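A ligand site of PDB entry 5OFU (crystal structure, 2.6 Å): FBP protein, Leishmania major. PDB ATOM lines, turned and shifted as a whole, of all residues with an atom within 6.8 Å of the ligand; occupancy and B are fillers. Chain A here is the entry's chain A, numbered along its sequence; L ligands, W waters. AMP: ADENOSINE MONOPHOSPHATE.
Water W2 lies within hydrogen-bond range of O1P of the ligand (2.8 Å), N of Thr 29 (3.0 Å), OE1 of Gln 20 (3.3 Å) and N of Gly 26 (3.5 Å).
A nitrogen (N1) of the ligand lies close to the backbone carbonyl oxygen (O) of Ser 19 (3.5 Å). Merely in contact with the ligand: Pro 21 (3.3 Å), Ser 24 (3.6 Å), Arg 140 (3.6 Å), Gln 20 (3.6 Å), Ser 183 (3.6 Å) and Val 166 (3.97 Å). Hydrophobic or aromatic side chains within 4 Å of the ligand: Ile 16, Pro 21, Phe 28, Tyr 113 and Val 166. 14 residues have an atom within 4 Å of the ligand: Ile 16, Ser 19, Gln 20, Pro 21, Ser 24, Arg 25, Gly 26, Asp 27, Phe 28, Thr 29, Tyr 113, Arg 140, Val 166 and Ser 183.
The backbone NH (N) of Arg 25 lies within hydrogen-bond range of an oxygen (O3P) of the ligand, at 2.7 Å. The guanidinium group (NH2) of Arg 25 lies within salt-bridge range of an oxygen (O2P) of the ligand (2.6 Å). O of Ile 16 is in hydrogen-bond range of N6 of the ligand, 2.7 Å away. An oxygen (O2P) of the ligand is in hydrogen-bond range of the side-chain hydroxyl (OH) of Tyr 113, 2.7 Å away. The side-chain hydroxyl of Thr 29 sits at hydrogen-bond distance from a nitrogen (N6) of the ligand. N of Asp 27 is in hydrogen-bond range of O1P of the ligand (3.1 Å). N of Phe 28 lies within hydrogen-bond range of O1P of the ligand (3.1 Å). N of Gly 26 is in hydrogen-bond range of O1P of the ligand (3.2 Å).
The guanidinium group (NH1) of Arg 25 lies within salt-bridge range of the side-chain carboxylate (OD2) of Asp 27, at 3.4 Å. The side-chain carboxylate (OD1) of Asp 112 lies within salt-bridge range of the guanidinium group (NH2) of Arg 25 (2.8 Å). The side-chain hydroxyl of Thr 29 sits at hydrogen-bond distance from the side-chain amide oxygen of Gln 20 (2.6 Å). OG of Ser 19 lies within hydrogen-bond range of O of Tyr 15, 2.7 Å away. The side-chain hydroxyl (OG) of Ser 24 is in hydrogen-bond range of the backbone carbonyl oxygen (O) of Pro 21. NE of Arg 140 is in salt-bridge range of OD2 of Asp 112.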
ATOM      1  N   TYR A  15      29.191 -25.446  26.933  1.00  0.00           N
ATOM      2  CA  TYR A  15      27.815 -25.597  27.357  1.00  0.00           C
ATOM      3  C   TYR A  15      27.075 -24.260  27.406  1.00  0.00           C
ATOM      4  O   TYR A  15      25.909 -24.186  26.984  1.00  0.00           O
ATOM      5  CB  TYR A  15      27.788 -26.296  28.733  1.00  0.00           C
ATOM      6  CG  TYR A  15      26.433 -26.426  29.386  1.00  0.00           C
ATOM      7  CD1 TYR A  15      25.964 -25.438  30.262  1.00  0.00           C
ATOM      8  CD2 TYR A  15      25.628 -27.545  29.160  1.00  0.00           C
ATOM      9  CE1 TYR A  15      24.735 -25.557  30.873  1.00  0.00           C
ATOM     10  CE2 TYR A  15      24.385 -27.669  29.764  1.00  0.00           C
ATOM     11  CZ  TYR A  15      23.949 -26.676  30.620  1.00  0.00           C
ATOM     12  OH  TYR A  15      22.719 -26.792  31.247  1.00  0.00           O
ATOM     13  N   ILE A  16      27.719 -23.221  27.945  1.00  0.00           N
ATOM     14  CA  ILE A  16      27.100 -21.903  28.088  1.00  0.00           C
ATOM     15  C   ILE A  16      26.810 -21.301  26.716  1.00  0.00           C
ATOM     16  O   ILE A  16      25.693 -20.844  26.459  1.00  0.00           O
ATOM     17  CB  ILE A  16      27.974 -20.940  28.921  1.00  0.00           C
ATOM     18  CG1 ILE A  16      27.983 -21.356  30.398  1.00  0.00           C
ATOM     19  CG2 ILE A  16      27.455 -19.504  28.832  1.00  0.00           C
ATOM     20  CD1 ILE A  16      29.159 -20.812  31.164  1.00  0.00           C
ATOM     21  N   ILE A  17      27.812 -21.314  25.848  1.00  0.00           N
ATOM     22  CA  ILE A  17      27.657 -20.773  24.508  1.00  0.00           C
ATOM     23  C   ILE A  17      26.613 -21.539  23.694  1.00  0.00           C
ATOM     24  O   ILE A  17      25.750 -20.918  23.081  1.00  0.00           O
ATOM     25  CB  ILE A  17      29.008 -20.727  23.753  1.00  0.00           C
ATOM     26  CG1 ILE A  17      29.905 -19.666  24.398  1.00  0.00           C
ATOM     27  CG2 ILE A  17      28.804 -20.387  22.289  1.00  0.00           C
ATOM     28  CD1 ILE A  17      31.376 -19.841  24.108  1.00  0.00           C
ATOM     29  N   LYS A  18      26.669 -22.867  23.713  1.00  0.00           N
ATOM     30  CA  LYS A  18      25.676 -23.691  23.005  1.00  0.00           C
ATOM     31  C   LYS A  18      24.245 -23.562  23.539  1.00  0.00           C
ATOM     32  O   LYS A  18      23.310 -23.881  22.829  1.00  0.00           O
ATOM     33  CB  LYS A  18      26.089 -25.167  22.956  1.00  0.00           C
ATOM     34  CG  LYS A  18      27.122 -25.436  21.887  1.00  0.00           C
ATOM     35  CD  LYS A  18      27.789 -26.792  22.042  1.00  0.00           C
ATOM     36  CE  LYS A  18      28.911 -26.955  21.026  1.00  0.00           C
ATOM     37  NZ  LYS A  18      29.735 -28.165  21.292  1.00  0.00           N
ATOM     38  N   SER A  19      24.102 -23.159  24.804  1.00  0.00           N
ATOM     39  CA  SER A  19      22.791 -22.931  25.419  1.00  0.00           C
ATOM     40  C   SER A  19      22.185 -21.576  25.058  1.00  0.00           C
ATOM     41  O   SER A  19      21.018 -21.351  25.352  1.00  0.00           O
ATOM     42  CB  SER A  19      22.873 -23.027  26.951  1.00  0.00           C
ATOM     43  OG  SER A  19      23.277 -24.327  27.381  1.00  0.00           O
ATOM     44  N   GLN A  20      22.962 -20.681  24.451  1.00  0.00           N
ATOM     45  CA  GLN A  20      22.458 -19.334  24.120  1.00  0.00           C
ATOM     46  C   GLN A  20      21.340 -19.410  23.058  1.00  0.00           C
ATOM     47  O   GLN A  20      21.615 -19.848  21.938  1.00  0.00           O
ATOM     48  CB  GLN A  20      23.592 -18.433  23.590  1.00  0.00           C
ATOM     49  CG  GLN A  20      23.258 -16.960  23.690  1.00  0.00           C
ATOM     50  CD  GLN A  20      24.415 -16.046  23.314  1.00  0.00           C
ATOM     51  OE1 GLN A  20      25.541 -16.025  23.902  1.00  0.00           O
ATOM     52  NE2 GLN A  20      24.137 -15.283  22.301  1.00  0.00           N
ATOM     53  N   PRO A  21      20.092 -19.022  23.411  1.00  0.00           N
ATOM     54  CA  PRO A  21      19.027 -19.055  22.405  1.00  0.00           C
ATOM     55  C   PRO A  21      19.308 -18.098  21.247  1.00  0.00           C
ATOM     56  O   PRO A  21      19.987 -17.086  21.458  1.00  0.00           O
ATOM     57  CB  PRO A  21      17.794 -18.579  23.180  1.00  0.00           C
ATOM     58  CG  PRO A  21      18.107 -18.861  24.602  1.00  0.00           C
ATOM     59  CD  PRO A  21      19.578 -18.580  24.718  1.00  0.00           C
ATOM     60  N   HIS A  23      18.896 -14.993  18.801  1.00  0.00           N
ATOM     61  CA  HIS A  23      18.492 -13.601  19.093  1.00  0.00           C
ATOM     62  C   HIS A  23      18.481 -13.264  20.593  1.00  0.00           C
ATOM     63  O   HIS A  23      17.511 -12.734  21.118  1.00  0.00           O
ATOM     64  CB  HIS A  23      17.143 -13.264  18.439  1.00  0.00           C
ATOM     65  CG  HIS A  23      17.153 -13.372  16.952  1.00  0.00           C
ATOM     66  ND1 HIS A  23      16.843 -12.312  16.125  1.00  0.00           N
ATOM     67  CD2 HIS A  23      17.440 -14.415  16.132  1.00  0.00           C
ATOM     68  CE1 HIS A  23      16.938 -12.698  14.863  1.00  0.00           C
ATOM     69  NE2 HIS A  23      17.307 -13.968  14.844  1.00  0.00           N
ATOM     70  N   SER A  24      19.584 -13.597  21.274  1.00  0.00           N
ATOM     71  CA  SER A  24      19.930 -13.081  22.586  1.00  0.00           C
ATOM     72  C   SER A  24      21.001 -12.006  22.393  1.00  0.00           C
ATOM     73  O   SER A  24      21.745 -12.036  21.412  1.00  0.00           O
ATOM     74  CB  SER A  24      20.481 -14.201  23.480  1.00  0.00           C
ATOM     75  OG  SER A  24      19.670 -15.356  23.426  1.00  0.00           O
ATOM     76  N   ARG A  25      21.093 -11.083  23.336  1.00  0.00           N
ATOM     77  CA  ARG A  25      22.110 -10.037  23.315  1.00  0.00           C
ATOM     78  C   ARG A  25      23.522 -10.532  23.599  1.00  0.00           C
ATOM     79  O   ARG A  25      24.508  -9.887  23.212  1.00  0.00           O
ATOM     80  CB  ARG A  25      21.765  -8.957  24.334  1.00  0.00           C
ATOM     81  CG  ARG A  25      20.479  -8.222  24.020  1.00  0.00           C
ATOM     82  CD  ARG A  25      20.008  -7.408  25.216  1.00  0.00           C
ATOM     83  NE  ARG A  25      19.743  -8.273  26.363  1.00  0.00           N
ATOM     84  CZ  ARG A  25      19.442  -7.849  27.590  1.00  0.00           C
ATOM     85  NH1 ARG A  25      19.365  -6.551  27.853  1.00  0.00           N
ATOM     86  NH2 ARG A  25      19.230  -8.734  28.551  1.00  0.00           N
ATOM     87  N   GLY A  26      23.625 -11.673  24.267  1.00  0.00           N
ATOM     88  CA  GLY A  26      24.902 -12.216  24.742  1.00  0.00           C
ATOM     89  C   GLY A  26      25.264 -11.784  26.155  1.00  0.00           C
ATOM     90  O   GLY A  26      26.331 -12.151  26.638  1.00  0.00           O
ATOM     91  N   ASP A  27      24.410 -10.987  26.810  1.00  0.00           N
ATOM     92  CA  ASP A  27      24.688 -10.434  28.137  1.00  0.00           C
ATOM     93  C   ASP A  27      24.706 -11.534  29.190  1.00  0.00           C
ATOM     94  O   ASP A  27      25.593 -11.580  30.045  1.00  0.00           O
ATOM     95  CB  ASP A  27      23.633  -9.413  28.578  1.00  0.00           C
ATOM     96  CG  ASP A  27      23.620  -8.149  27.741  1.00  0.00           C
ATOM     97  OD1 ASP A  27      24.501  -7.995  26.867  1.00  0.00           O
ATOM     98  OD2 ASP A  27      22.715  -7.316  27.964  1.00  0.00           O
ATOM     99  N   PHE A  28      23.717 -12.410  29.102  1.00  0.00           N
ATOM    100  CA  PHE A  28      23.596 -13.538  30.004  1.00  0.00           C
ATOM    101  C   PHE A  28      24.807 -14.464  29.851  1.00  0.00           C
ATOM    102  O   PHE A  28      25.338 -14.930  30.859  1.00  0.00           O
ATOM    103  CB  PHE A  28      22.300 -14.302  29.738  1.00  0.00           C
ATOM    104  CG  PHE A  28      22.050 -15.416  30.700  1.00  0.00           C
ATOM    105  CD1 PHE A  28      22.584 -16.680  30.472  1.00  0.00           C
ATOM    106  CD2 PHE A  28      21.270 -15.218  31.833  1.00  0.00           C
ATOM    107  CE1 PHE A  28      22.342 -17.713  31.354  1.00  0.00           C
ATOM    108  CE2 PHE A  28      21.019 -16.261  32.715  1.00  0.00           C
ATOM    109  CZ  PHE A  28      21.557 -17.510  32.480  1.00  0.00           C
ATOM    110  N   THR A  29      25.221 -14.723  28.614  1.00  0.00           N
ATOM    111  CA  THR A  29      26.423 -15.531  28.359  1.00  0.00           C
ATOM    112  C   THR A  29      27.651 -14.911  28.998  1.00  0.00           C
ATOM    113  O   THR A  29      28.393 -15.613  29.703  1.00  0.00           O
ATOM    114  CB  THR A  29      26.642 -15.783  26.870  1.00  0.00           C
ATOM    115  OG1 THR A  29      25.672 -16.742  26.434  1.00  0.00           O
ATOM    116  CG2 THR A  29      28.037 -16.348  26.581  1.00  0.00           C
ATOM    117  N   LEU A  30      27.830 -13.609  28.837  1.00  0.00           N
ATOM    118  CA  LEU A  30      28.946 -12.918  29.502  1.00  0.00           C
ATOM    119  C   LEU A  30      28.904 -12.942  31.042  1.00  0.00           C
ATOM    120  O   LEU A  30      29.936 -12.930  31.705  1.00  0.00           O
ATOM    121  CB  LEU A  30      29.089 -11.484  29.009  1.00  0.00           C
ATOM    122  CG  LEU A  30      29.658 -11.356  27.592  1.00  0.00           C
ATOM    123  CD1 LEU A  30      29.675  -9.894  27.151  1.00  0.00           C
ATOM    124  CD2 LEU A  30      31.050 -11.975  27.532  1.00  0.00           C
ATOM    125  N   MET A  32      27.558 -15.473  32.897  1.00  0.00           N
ATOM    126  CA  MET A  32      27.974 -16.831  33.256  1.00  0.00           C
ATOM    127  C   MET A  32      29.484 -17.012  33.179  1.00  0.00           C
ATOM    128  O   MET A  32      30.073 -17.648  34.033  1.00  0.00           O
ATOM    129  CB  MET A  32      27.309 -17.857  32.345  1.00  0.00           C
ATOM    130  CG  MET A  32      25.794 -17.953  32.465  1.00  0.00           C
ATOM    131  SD  MET A  32      25.255 -18.433  34.115  1.00  0.00           S
ATOM    132  CE  MET A  32      24.691 -16.842  34.748  1.00  0.00           C
ATOM    133  N   ASP A 112      20.491  -5.390  32.545  1.00  0.00           N
ATOM    134  CA  ASP A 112      19.180  -5.485  33.202  1.00  0.00           C
ATOM    135  C   ASP A 112      19.065  -6.716  34.107  1.00  0.00           C
ATOM    136  O   ASP A 112      17.958  -7.165  34.383  1.00  0.00           O
ATOM    137  CB  ASP A 112      18.061  -5.430  32.149  1.00  0.00           C
ATOM    138  CG  ASP A 112      18.082  -6.621  31.213  1.00  0.00           C
ATOM    139  OD1 ASP A 112      19.178  -6.964  30.723  1.00  0.00           O
ATOM    140  OD2 ASP A 112      17.005  -7.203  30.939  1.00  0.00           O
ATOM    141  N   TYR A 113      20.208  -7.249  34.560  1.00  0.00           N
ATOM    142  CA  TYR A 113      20.237  -8.406  35.448  1.00  0.00           C
ATOM    143  C   TYR A 113      20.542  -7.987  36.882  1.00  0.00           C
ATOM    144  O   TYR A 113      21.366  -7.105  37.104  1.00  0.00           O
ATOM    145  CB  TYR A 113      21.248  -9.457  34.967  1.00  0.00           C
ATOM    146  CG  TYR A 113      20.766 -10.186  33.749  1.00  0.00           C
ATOM    147  CD1 TYR A 113      19.749 -11.116  33.853  1.00  0.00           C
ATOM    148  CD2 TYR A 113      21.312  -9.952  32.492  1.00  0.00           C
ATOM    149  CE1 TYR A 113      19.282 -11.800  32.746  1.00  0.00           C
ATOM    150  CE2 TYR A 113      20.848 -10.631  31.372  1.00  0.00           C
ATOM    151  CZ  TYR A 113      19.822 -11.558  31.498  1.00  0.00           C
ATOM    152  OH  TYR A 113      19.321 -12.247  30.412  1.00  0.00           O
ATOM    153  N   ARG A 140      15.897 -10.957  36.162  1.00  0.00           N
ATOM    154  CA  ARG A 140      15.816  -9.921  35.145  1.00  0.00           C
ATOM    155  C   ARG A 140      14.859  -8.817  35.591  1.00  0.00           C
ATOM    156  O   ARG A 140      13.845  -9.091  36.244  1.00  0.00           O
ATOM    157  CB  ARG A 140      15.355 -10.534  33.817  1.00  0.00           C
ATOM    158  CG  ARG A 140      15.861  -9.811  32.605  1.00  0.00           C
ATOM    159  CD  ARG A 140      15.606 -10.580  31.324  1.00  0.00           C
ATOM    160  NE  ARG A 140      15.936  -9.749  30.179  1.00  0.00           N
ATOM    161  CZ  ARG A 140      15.808 -10.127  28.904  1.00  0.00           C
ATOM    162  NH1 ARG A 140      15.336 -11.331  28.582  1.00  0.00           N
ATOM    163  NH2 ARG A 140      16.158  -9.277  27.946  1.00  0.00           N
ATOM    164  N   VAL A 166      15.718 -16.169  36.395  1.00  0.00           N
ATOM    165  CA  VAL A 166      16.200 -16.725  35.125  1.00  0.00           C
ATOM    166  C   VAL A 166      17.287 -17.784  35.294  1.00  0.00           C
ATOM    167  O   VAL A 166      17.419 -18.661  34.437  1.00  0.00           O
ATOM    168  CB  VAL A 166      16.663 -15.631  34.136  1.00  0.00           C
ATOM    169  CG1 VAL A 166      15.588 -14.559  34.008  1.00  0.00           C
ATOM    170  CG2 VAL A 166      17.969 -14.982  34.546  1.00  0.00           C
ATOM    171  N   SER A 167      18.070 -17.718  36.370  1.00  0.00           N
ATOM    172  CA  SER A 167      19.196 -18.632  36.596  1.00  0.00           C
ATOM    173  C   SER A 167      19.575 -18.756  38.064  1.00  0.00           C
ATOM    174  O   SER A 167      19.436 -17.803  38.834  1.00  0.00           O
ATOM    175  CB  SER A 167      20.410 -18.150  35.815  1.00  0.00           C
ATOM    176  OG  SER A 167      21.411 -19.148  35.767  1.00  0.00           O
ATOM    177  N   SER A 183      19.245 -23.014  34.080  1.00  0.00           N
ATOM    178  CA  SER A 183      18.579 -21.887  33.422  1.00  0.00           C
ATOM    179  C   SER A 183      17.079 -22.152  33.187  1.00  0.00           C
ATOM    180  O   SER A 183      16.470 -21.570  32.288  1.00  0.00           O
ATOM    181  CB  SER A 183      19.225 -21.602  32.070  1.00  0.00           C
ATOM    182  OG  SER A 183      20.632 -21.587  32.156  1.00  0.00           O
ATOM    183  N   HIS A 185      15.902 -25.327  32.513  1.00  0.00           N
ATOM    184  CA  HIS A 185      15.770 -26.554  31.704  1.00  0.00           C
ATOM    185  C   HIS A 185      16.615 -27.672  32.309  1.00  0.00           C
ATOM    186  O   HIS A 185      17.454 -28.258  31.639  1.00  0.00           O
ATOM    187  CB  HIS A 185      16.193 -26.278  30.260  1.00  0.00           C
ATOM    188  CG  HIS A 185      15.389 -25.216  29.594  1.00  0.00           C
ATOM    189  ND1 HIS A 185      15.798 -23.899  29.537  1.00  0.00           N
ATOM    190  CD2 HIS A 185      14.170 -25.256  29.006  1.00  0.00           C
ATOM    191  CE1 HIS A 185      14.876 -23.181  28.928  1.00  0.00           C
ATOM    192  NE2 HIS A 185      13.875 -23.982  28.593  1.00  0.00           N
HETATM  193  P   AMP L   1      20.365 -11.985  26.940  1.00  0.00           P
HETATM  194  O1P AMP L   1      21.753 -12.524  26.740  1.00  0.00           O
HETATM  195  O2P AMP L   1      20.194 -11.105  28.154  1.00  0.00           O
HETATM  196  O3P AMP L   1      19.732 -11.383  25.704  1.00  0.00           O
HETATM  197  O5' AMP L   1      19.515 -13.322  27.162  1.00  0.00           O
HETATM  198  C5' AMP L   1      18.127 -13.275  27.480  1.00  0.00           C
HETATM  199  C4' AMP L   1      17.634 -14.600  28.027  1.00  0.00           C
HETATM  200  O4' AMP L   1      17.925 -15.674  27.131  1.00  0.00           O
HETATM  201  C3' AMP L   1      18.268 -14.987  29.350  1.00  0.00           C
HETATM  202  O3' AMP L   1      17.582 -14.426  30.467  1.00  0.00           O
HETATM  203  C2' AMP L   1      18.199 -16.493  29.339  1.00  0.00           C
HETATM  204  O2' AMP L   1      16.961 -16.981  29.833  1.00  0.00           O
HETATM  205  C1' AMP L   1      18.368 -16.824  27.866  1.00  0.00           C
HETATM  206  N9  AMP L   1      19.817 -17.089  27.634  1.00  0.00           N
HETATM  207  C8  AMP L   1      20.731 -16.251  27.099  1.00  0.00           C
HETATM  208  N7  AMP L   1      21.949 -16.817  27.058  1.00  0.00           N
HETATM  209  C5  AMP L   1      21.843 -18.037  27.583  1.00  0.00           C
HETATM  210  C6  AMP L   1      22.762 -19.151  27.851  1.00  0.00           C
HETATM  211  N6  AMP L   1      24.059 -19.031  27.520  1.00  0.00           N
HETATM  212  N1  AMP L   1      22.269 -20.266  28.427  1.00  0.00           N
HETATM  213  C2  AMP L   1      20.959 -20.383  28.756  1.00  0.00           C
HETATM  214  N3  AMP L   1      20.061 -19.391  28.550  1.00  0.00           N
HETATM  215  C4  AMP L   1      20.441 -18.225  27.976  1.00  0.00           C
HETATM  216  O   HOH W   1      24.217 -21.789  30.378  1.00  0.00           O
HETATM  217  O   HOH W   2      23.503 -14.624  26.122  1.00  0.00           O
